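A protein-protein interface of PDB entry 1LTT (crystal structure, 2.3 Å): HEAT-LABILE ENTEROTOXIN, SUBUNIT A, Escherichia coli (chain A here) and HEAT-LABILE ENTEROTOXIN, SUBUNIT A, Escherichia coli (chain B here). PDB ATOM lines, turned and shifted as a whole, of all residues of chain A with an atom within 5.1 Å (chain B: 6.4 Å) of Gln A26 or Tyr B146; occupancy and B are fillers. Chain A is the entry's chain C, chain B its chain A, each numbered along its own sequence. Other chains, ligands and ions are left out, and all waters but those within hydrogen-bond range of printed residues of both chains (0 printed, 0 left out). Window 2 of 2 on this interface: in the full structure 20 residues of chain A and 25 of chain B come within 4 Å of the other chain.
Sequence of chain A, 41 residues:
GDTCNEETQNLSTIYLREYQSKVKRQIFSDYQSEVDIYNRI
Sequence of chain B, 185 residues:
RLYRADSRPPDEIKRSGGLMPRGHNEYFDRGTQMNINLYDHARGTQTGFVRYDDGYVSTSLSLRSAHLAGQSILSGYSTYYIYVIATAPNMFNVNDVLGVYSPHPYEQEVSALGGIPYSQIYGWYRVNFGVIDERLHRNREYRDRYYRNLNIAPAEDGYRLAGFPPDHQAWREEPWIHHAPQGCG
The guanidinium group (NH2) of Arg B143 lies within hydrogen-bond range of the backbone carbonyl oxygen (O) of Gln A26 (3.3 Å). OH of Tyr A19 lies within hydrogen-bond range of OH of Tyr B147 (2.8 Å). The guanidinium group (NH1) of Arg B143 is in salt-bridge range of the side-chain carboxylate (OD2) of Asp A30.
OD1 of Asn B149 sits close to O of Tyr B146, at 3.0 Å. N of Arg B143 lies within hydrogen-bond range of O of Ser B119 (3.0 Å).
Among the printed residues, merely in contact across the chains: Gln A26 with Tyr B146, Lys A22 with Tyr B146, Tyr A19 with Ala B88, Ile A27 with Arg B143 and Val A23 with Tyr B147.
Printed residues of chain B within 4 Å of Lys A22: Tyr B146. Printed residues of chain B within 4 Å of Val A23: Tyr B147 (3.9 Å). Of chain A, only Lys A22 and Gln A26 come within 4 Å of Tyr B146. The nearest residue of chain B that does not touch Gln A26 is Ser B119 (5.9 Å).
Printed residues of chain B that touch a printed residue of chain A: Ala B88, Arg B143, Tyr B146 and Tyr B147. Hydrophobic or aromatic side chains of chain B that line the printed part of chain A: Ala B88, Tyr B146 and Tyr B147. Hydrophobic or aromatic side chains of chain A that line the printed part of chain B: Tyr A19, Val A23 and Ile A27. Along chain A the printed residues that touch a printed residue of chain B span positions 19 to 30. Among the printed residues, Asp or Glu carboxylates within 4 Å of a Lys or Arg side-chain nitrogen of the other chain: Asp A30 with Arg B143 (2.9 Å).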
ATOM      1  N   TYR A  19      -1.767  18.139  -4.062  1.00  0.00           N
ATOM      2  CA  TYR A  19      -3.060  18.538  -3.502  1.00  0.00           C
ATOM      3  C   TYR A  19      -3.978  18.894  -4.679  1.00  0.00           C
ATOM      4  O   TYR A  19      -5.160  18.518  -4.680  1.00  0.00           O
ATOM      5  CB  TYR A  19      -2.889  19.743  -2.538  1.00  0.00           C
ATOM      6  CG  TYR A  19      -4.214  20.182  -1.912  1.00  0.00           C
ATOM      7  CD1 TYR A  19      -4.813  19.449  -0.898  1.00  0.00           C
ATOM      8  CD2 TYR A  19      -4.880  21.295  -2.390  1.00  0.00           C
ATOM      9  CE1 TYR A  19      -6.056  19.798  -0.374  1.00  0.00           C
ATOM     10  CE2 TYR A  19      -6.118  21.651  -1.868  1.00  0.00           C
ATOM     11  CZ  TYR A  19      -6.702  20.898  -0.867  1.00  0.00           C
ATOM     12  OH  TYR A  19      -7.958  21.209  -0.383  1.00  0.00           O
ATOM     13  N   LYS A  22      -5.875  16.084  -5.966  1.00  0.00           N
ATOM     14  CA  LYS A  22      -6.998  15.688  -5.118  1.00  0.00           C
ATOM     15  C   LYS A  22      -8.240  16.490  -5.399  1.00  0.00           C
ATOM     16  O   LYS A  22      -9.331  15.940  -5.511  1.00  0.00           O
ATOM     17  CB  LYS A  22      -6.645  15.851  -3.650  1.00  0.00           C
ATOM     18  CG  LYS A  22      -5.619  14.805  -3.244  1.00  0.00           C
ATOM     19  CD  LYS A  22      -6.119  13.422  -3.715  1.00  0.00           C
ATOM     20  CE  LYS A  22      -5.146  12.229  -3.581  1.00  0.00           C
ATOM     21  NZ  LYS A  22      -4.962  11.781  -2.208  1.00  0.00           N
ATOM     22  N   VAL A  23      -8.054  17.789  -5.585  1.00  0.00           N
ATOM     23  CA  VAL A  23      -9.124  18.724  -5.962  1.00  0.00           C
ATOM     24  C   VAL A  23      -9.655  18.402  -7.366  1.00  0.00           C
ATOM     25  O   VAL A  23     -10.877  18.359  -7.555  1.00  0.00           O
ATOM     26  CB  VAL A  23      -8.576  20.186  -5.891  1.00  0.00           C
ATOM     27  CG1 VAL A  23      -9.588  21.218  -6.315  1.00  0.00           C
ATOM     28  CG2 VAL A  23      -8.232  20.501  -4.450  1.00  0.00           C
ATOM     29  N   LYS A  24      -8.821  18.105  -8.361  1.00  0.00           N
ATOM     30  CA  LYS A  24      -9.319  17.762  -9.690  1.00  0.00           C
ATOM     31  C   LYS A  24     -10.121  16.466  -9.666  1.00  0.00           C
ATOM     32  O   LYS A  24     -11.151  16.356 -10.321  1.00  0.00           O
ATOM     33  CB  LYS A  24      -8.165  17.624 -10.668  1.00  0.00           C
ATOM     34  CG  LYS A  24      -7.737  18.979 -11.139  1.00  0.00           C
ATOM     35  CD  LYS A  24      -6.540  18.733 -12.068  1.00  0.00           C
ATOM     36  CE  LYS A  24      -6.095  20.047 -12.714  1.00  0.00           C
ATOM     37  NZ  LYS A  24      -4.979  19.784 -13.589  1.00  0.00           N
ATOM     38  N   ARG A  25      -9.707  15.484  -8.863  1.00  0.00           N
ATOM     39  CA  ARG A  25     -10.462  14.238  -8.660  1.00  0.00           C
ATOM     40  C   ARG A  25     -11.859  14.530  -8.099  1.00  0.00           C
ATOM     41  O   ARG A  25     -12.811  13.860  -8.476  1.00  0.00           O
ATOM     42  CB  ARG A  25      -9.668  13.339  -7.721  1.00  0.00           C
ATOM     43  CG  ARG A  25      -8.510  12.624  -8.407  1.00  0.00           C
ATOM     44  CD  ARG A  25      -7.583  11.971  -7.376  1.00  0.00           C
ATOM     45  NE  ARG A  25      -8.260  10.875  -6.697  1.00  0.00           N
ATOM     46  CZ  ARG A  25      -7.593   9.865  -6.110  1.00  0.00           C
ATOM     47  NH1 ARG A  25      -6.267   9.821  -6.101  1.00  0.00           N
ATOM     48  NH2 ARG A  25      -8.244   8.825  -5.581  1.00  0.00           N
ATOM     49  N   GLN A  26     -12.044  15.571  -7.282  1.00  0.00           N
ATOM     50  CA  GLN A  26     -13.355  15.962  -6.813  1.00  0.00           C
ATOM     51  C   GLN A  26     -14.142  16.673  -7.873  1.00  0.00           C
ATOM     52  O   GLN A  26     -15.197  16.199  -8.285  1.00  0.00           O
ATOM     53  CB  GLN A  26     -13.306  16.912  -5.608  1.00  0.00           C
ATOM     54  CG  GLN A  26     -12.764  16.240  -4.354  1.00  0.00           C
ATOM     55  CD  GLN A  26     -13.552  15.000  -3.958  1.00  0.00           C
ATOM     56  OE1 GLN A  26     -14.751  15.080  -3.682  1.00  0.00           O
ATOM     57  NE2 GLN A  26     -12.946  13.827  -3.884  1.00  0.00           N
ATOM     58  N   ILE A  27     -13.640  17.795  -8.370  1.00  0.00           N
ATOM     59  CA  ILE A  27     -14.463  18.604  -9.231  1.00  0.00           C
ATOM     60  C   ILE A  27     -14.556  18.128 -10.648  1.00  0.00           C
ATOM     61  O   ILE A  27     -15.616  18.295 -11.260  1.00  0.00           O
ATOM     62  CB  ILE A  27     -13.966  20.048  -9.150  1.00  0.00           C
ATOM     63  CG1 ILE A  27     -12.546  20.222  -9.566  1.00  0.00           C
ATOM     64  CG2 ILE A  27     -14.069  20.467  -7.670  1.00  0.00           C
ATOM     65  CD1 ILE A  27     -12.011  21.647  -9.323  1.00  0.00           C
ATOM     66  N   PHE A  28     -13.554  17.465 -11.226  1.00  0.00           N
ATOM     67  CA  PHE A  28     -13.677  16.974 -12.593  1.00  0.00           C
ATOM     68  C   PHE A  28     -14.493  15.704 -12.716  1.00  0.00           C
ATOM     69  O   PHE A  28     -15.157  15.476 -13.724  1.00  0.00           O
ATOM     70  CB  PHE A  28     -12.291  16.757 -13.173  1.00  0.00           C
ATOM     71  CG  PHE A  28     -11.529  18.032 -13.522  1.00  0.00           C
ATOM     72  CD1 PHE A  28     -12.030  19.298 -13.201  1.00  0.00           C
ATOM     73  CD2 PHE A  28     -10.305  17.914 -14.150  1.00  0.00           C
ATOM     74  CE1 PHE A  28     -11.317  20.451 -13.493  1.00  0.00           C
ATOM     75  CE2 PHE A  28      -9.593  19.056 -14.442  1.00  0.00           C
ATOM     76  CZ  PHE A  28     -10.091  20.314 -14.113  1.00  0.00           C
ATOM     77  N   SER A  29     -14.524  14.864 -11.689  1.00  0.00           N
ATOM     78  CA  SER A  29     -15.347  13.673 -11.648  1.00  0.00           C
ATOM     79  C   SER A  29     -16.820  13.916 -11.827  1.00  0.00           C
ATOM     80  O   SER A  29     -17.497  13.014 -12.344  1.00  0.00           O
ATOM     81  CB  SER A  29     -15.138  12.971 -10.349  1.00  0.00           C
ATOM     82  OG  SER A  29     -13.892  12.297 -10.492  1.00  0.00           O
ATOM     83  N   ASP A  30     -17.318  15.096 -11.420  1.00  0.00           N
ATOM     84  CA  ASP A  30     -18.702  15.494 -11.693  1.00  0.00           C
ATOM     85  C   ASP A  30     -19.129  15.513 -13.153  1.00  0.00           C
ATOM     86  O   ASP A  30     -20.334  15.453 -13.413  1.00  0.00           O
ATOM     87  CB  ASP A  30     -19.032  16.888 -11.221  1.00  0.00           C
ATOM     88  CG  ASP A  30     -18.981  17.111  -9.725  1.00  0.00           C
ATOM     89  OD1 ASP A  30     -18.768  16.155  -8.977  1.00  0.00           O
ATOM     90  OD2 ASP A  30     -19.162  18.269  -9.322  1.00  0.00           O
ATOM     91  N   ALA B  88      -7.841  21.742   5.705  1.00  0.00           N
ATOM     92  CA  ALA B  88      -7.475  20.694   4.771  1.00  0.00           C
ATOM     93  C   ALA B  88      -5.943  20.658   4.765  1.00  0.00           C
ATOM     94  O   ALA B  88      -5.339  21.663   5.160  1.00  0.00           O
ATOM     95  CB  ALA B  88      -7.994  21.022   3.339  1.00  0.00           C
ATOM     96  N   SER B 119     -13.788  25.424  -4.044  1.00  0.00           N
ATOM     97  CA  SER B 119     -14.572  24.381  -3.389  1.00  0.00           C
ATOM     98  C   SER B 119     -14.312  24.163  -1.881  1.00  0.00           C
ATOM     99  O   SER B 119     -15.055  23.447  -1.198  1.00  0.00           O
ATOM    100  CB  SER B 119     -14.326  23.099  -4.193  1.00  0.00           C
ATOM    101  OG  SER B 119     -12.959  22.699  -4.355  1.00  0.00           O
ATOM    102  N   ARG B 143     -17.375  21.577  -1.248  1.00  0.00           N
ATOM    103  CA  ARG B 143     -17.520  20.121  -1.255  1.00  0.00           C
ATOM    104  C   ARG B 143     -17.622  19.642   0.182  1.00  0.00           C
ATOM    105  O   ARG B 143     -16.642  19.350   0.873  1.00  0.00           O
ATOM    106  CB  ARG B 143     -16.339  19.384  -1.875  1.00  0.00           C
ATOM    107  CG  ARG B 143     -15.845  19.770  -3.257  1.00  0.00           C
ATOM    108  CD  ARG B 143     -16.816  19.670  -4.413  1.00  0.00           C
ATOM    109  NE  ARG B 143     -17.058  18.293  -4.798  1.00  0.00           N
ATOM    110  CZ  ARG B 143     -17.453  17.982  -6.034  1.00  0.00           C
ATOM    111  NH1 ARG B 143     -17.634  18.904  -6.977  1.00  0.00           N
ATOM    112  NH2 ARG B 143     -17.727  16.713  -6.291  1.00  0.00           N
ATOM    113  N   ASP B 144     -18.846  19.582   0.668  1.00  0.00           N
ATOM    114  CA  ASP B 144     -19.099  19.127   2.020  1.00  0.00           C
ATOM    115  C   ASP B 144     -18.663  17.701   2.321  1.00  0.00           C
ATOM    116  O   ASP B 144     -18.064  17.539   3.366  1.00  0.00           O
ATOM    117  CB  ASP B 144     -20.583  19.269   2.343  1.00  0.00           C
ATOM    118  CG  ASP B 144     -20.947  18.954   3.809  1.00  0.00           C
ATOM    119  OD1 ASP B 144     -20.495  19.665   4.704  1.00  0.00           O
ATOM    120  OD2 ASP B 144     -21.690  18.001   4.054  1.00  0.00           O
ATOM    121  N   ARG B 145     -18.841  16.652   1.522  1.00  0.00           N
ATOM    122  CA  ARG B 145     -18.451  15.356   1.966  1.00  0.00           C
ATOM    123  C   ARG B 145     -16.942  15.271   1.942  1.00  0.00           C
ATOM    124  O   ARG B 145     -16.361  14.641   2.834  1.00  0.00           O
ATOM    125  CB  ARG B 145     -19.039  14.265   1.066  1.00  0.00           C
ATOM    126  CG  ARG B 145     -18.764  12.832   1.619  1.00  0.00           C
ATOM    127  CD  ARG B 145     -19.008  11.779   0.548  1.00  0.00           C
ATOM    128  NE  ARG B 145     -20.439  11.610   0.313  1.00  0.00           N
ATOM    129  CZ  ARG B 145     -21.022  11.803  -0.879  1.00  0.00           C
ATOM    130  NH1 ARG B 145     -20.335  12.182  -1.968  1.00  0.00           N
ATOM    131  NH2 ARG B 145     -22.327  11.594  -0.967  1.00  0.00           N
ATOM    132  N   TYR B 146     -16.274  15.924   0.998  1.00  0.00           N
ATOM    133  CA  TYR B 146     -14.843  15.807   0.962  1.00  0.00           C
ATOM    134  C   TYR B 146     -14.163  16.497   2.138  1.00  0.00           C
ATOM    135  O   TYR B 146     -13.338  15.901   2.837  1.00  0.00           O
ATOM    136  CB  TYR B 146     -14.299  16.386  -0.341  1.00  0.00           C
ATOM    137  CG  TYR B 146     -12.796  16.130  -0.507  1.00  0.00           C
ATOM    138  CD1 TYR B 146     -12.324  14.864  -0.803  1.00  0.00           C
ATOM    139  CD2 TYR B 146     -11.888  17.169  -0.376  1.00  0.00           C
ATOM    140  CE1 TYR B 146     -10.964  14.644  -0.964  1.00  0.00           C
ATOM    141  CE2 TYR B 146     -10.519  16.944  -0.546  1.00  0.00           C
ATOM    142  CZ  TYR B 146     -10.069  15.676  -0.847  1.00  0.00           C
ATOM    143  OH  TYR B 146      -8.716  15.441  -1.064  1.00  0.00           O
ATOM    144  N   TYR B 147     -14.452  17.783   2.323  1.00  0.00           N
ATOM    145  CA  TYR B 147     -13.804  18.587   3.343  1.00  0.00           C
ATOM    146  C   TYR B 147     -14.263  18.309   4.761  1.00  0.00           C
ATOM    147  O   TYR B 147     -13.572  18.653   5.728  1.00  0.00           O
ATOM    148  CB  TYR B 147     -14.031  20.060   2.974  1.00  0.00           C
ATOM    149  CG  TYR B 147     -13.173  20.461   1.762  1.00  0.00           C
ATOM    150  CD1 TYR B 147     -11.800  20.393   1.907  1.00  0.00           C
ATOM    151  CD2 TYR B 147     -13.702  20.821   0.536  1.00  0.00           C
ATOM    152  CE1 TYR B 147     -10.951  20.668   0.854  1.00  0.00           C
ATOM    153  CE2 TYR B 147     -12.847  21.096  -0.531  1.00  0.00           C
ATOM    154  CZ  TYR B 147     -11.469  21.021  -0.371  1.00  0.00           C
ATOM    155  OH  TYR B 147     -10.556  21.288  -1.393  1.00  0.00           O
ATOM    156  N   ARG B 148     -15.390  17.599   4.884  1.00  0.00           N
ATOM    157  CA  ARG B 148     -16.079  17.342   6.139  1.00  0.00           C
ATOM    158  C   ARG B 148     -15.186  16.904   7.276  1.00  0.00           C
ATOM    159  O   ARG B 148     -15.302  17.348   8.417  1.00  0.00           O
ATOM    160  CB  ARG B 148     -17.152  16.268   5.921  1.00  0.00           C
ATOM    161  CG  ARG B 148     -18.205  16.074   7.012  1.00  0.00           C
ATOM    162  CD  ARG B 148     -19.226  15.017   6.607  1.00  0.00           C
ATOM    163  NE  ARG B 148     -20.110  15.480   5.539  1.00  0.00           N
ATOM    164  CZ  ARG B 148     -20.750  14.647   4.694  1.00  0.00           C
ATOM    165  NH1 ARG B 148     -20.623  13.319   4.765  1.00  0.00           N
ATOM    166  NH2 ARG B 148     -21.520  15.148   3.735  1.00  0.00           N
ATOM    167  N   ASN B 149     -14.248  16.067   6.915  1.00  0.00           N
ATOM    168  CA  ASN B 149     -13.413  15.383   7.862  1.00  0.00           C
ATOM    169  C   ASN B 149     -11.926  15.744   7.755  1.00  0.00           C
ATOM    170  O   ASN B 149     -11.119  15.057   8.385  1.00  0.00           O
ATOM    171  CB  ASN B 149     -13.662  13.901   7.603  1.00  0.00           C
ATOM    172  CG  ASN B 149     -13.309  13.521   6.132  1.00  0.00           C
ATOM    173  OD1 ASN B 149     -13.816  14.089   5.142  1.00  0.00           O
ATOM    174  ND2 ASN B 149     -12.412  12.558   5.917  1.00  0.00           N
ATOM    175  N   LEU B 150     -11.496  16.761   6.988  1.00  0.00           N
ATOM    176  CA  LEU B 150     -10.087  17.035   6.793  1.00  0.00           C
ATOM    177  C   LEU B 150      -9.563  18.041   7.786  1.00  0.00           C
ATOM    178  O   LEU B 150     -10.319  18.757   8.461  1.00  0.00           O
ATOM    179  CB  LEU B 150      -9.823  17.567   5.389  1.00  0.00           C
ATOM    180  CG  LEU B 150     -10.120  16.657   4.213  1.00  0.00           C
ATOM    181  CD1 LEU B 150      -9.523  17.283   2.984  1.00  0.00           C
ATOM    182  CD2 LEU B 150      -9.499  15.275   4.395  1.00  0.00           C
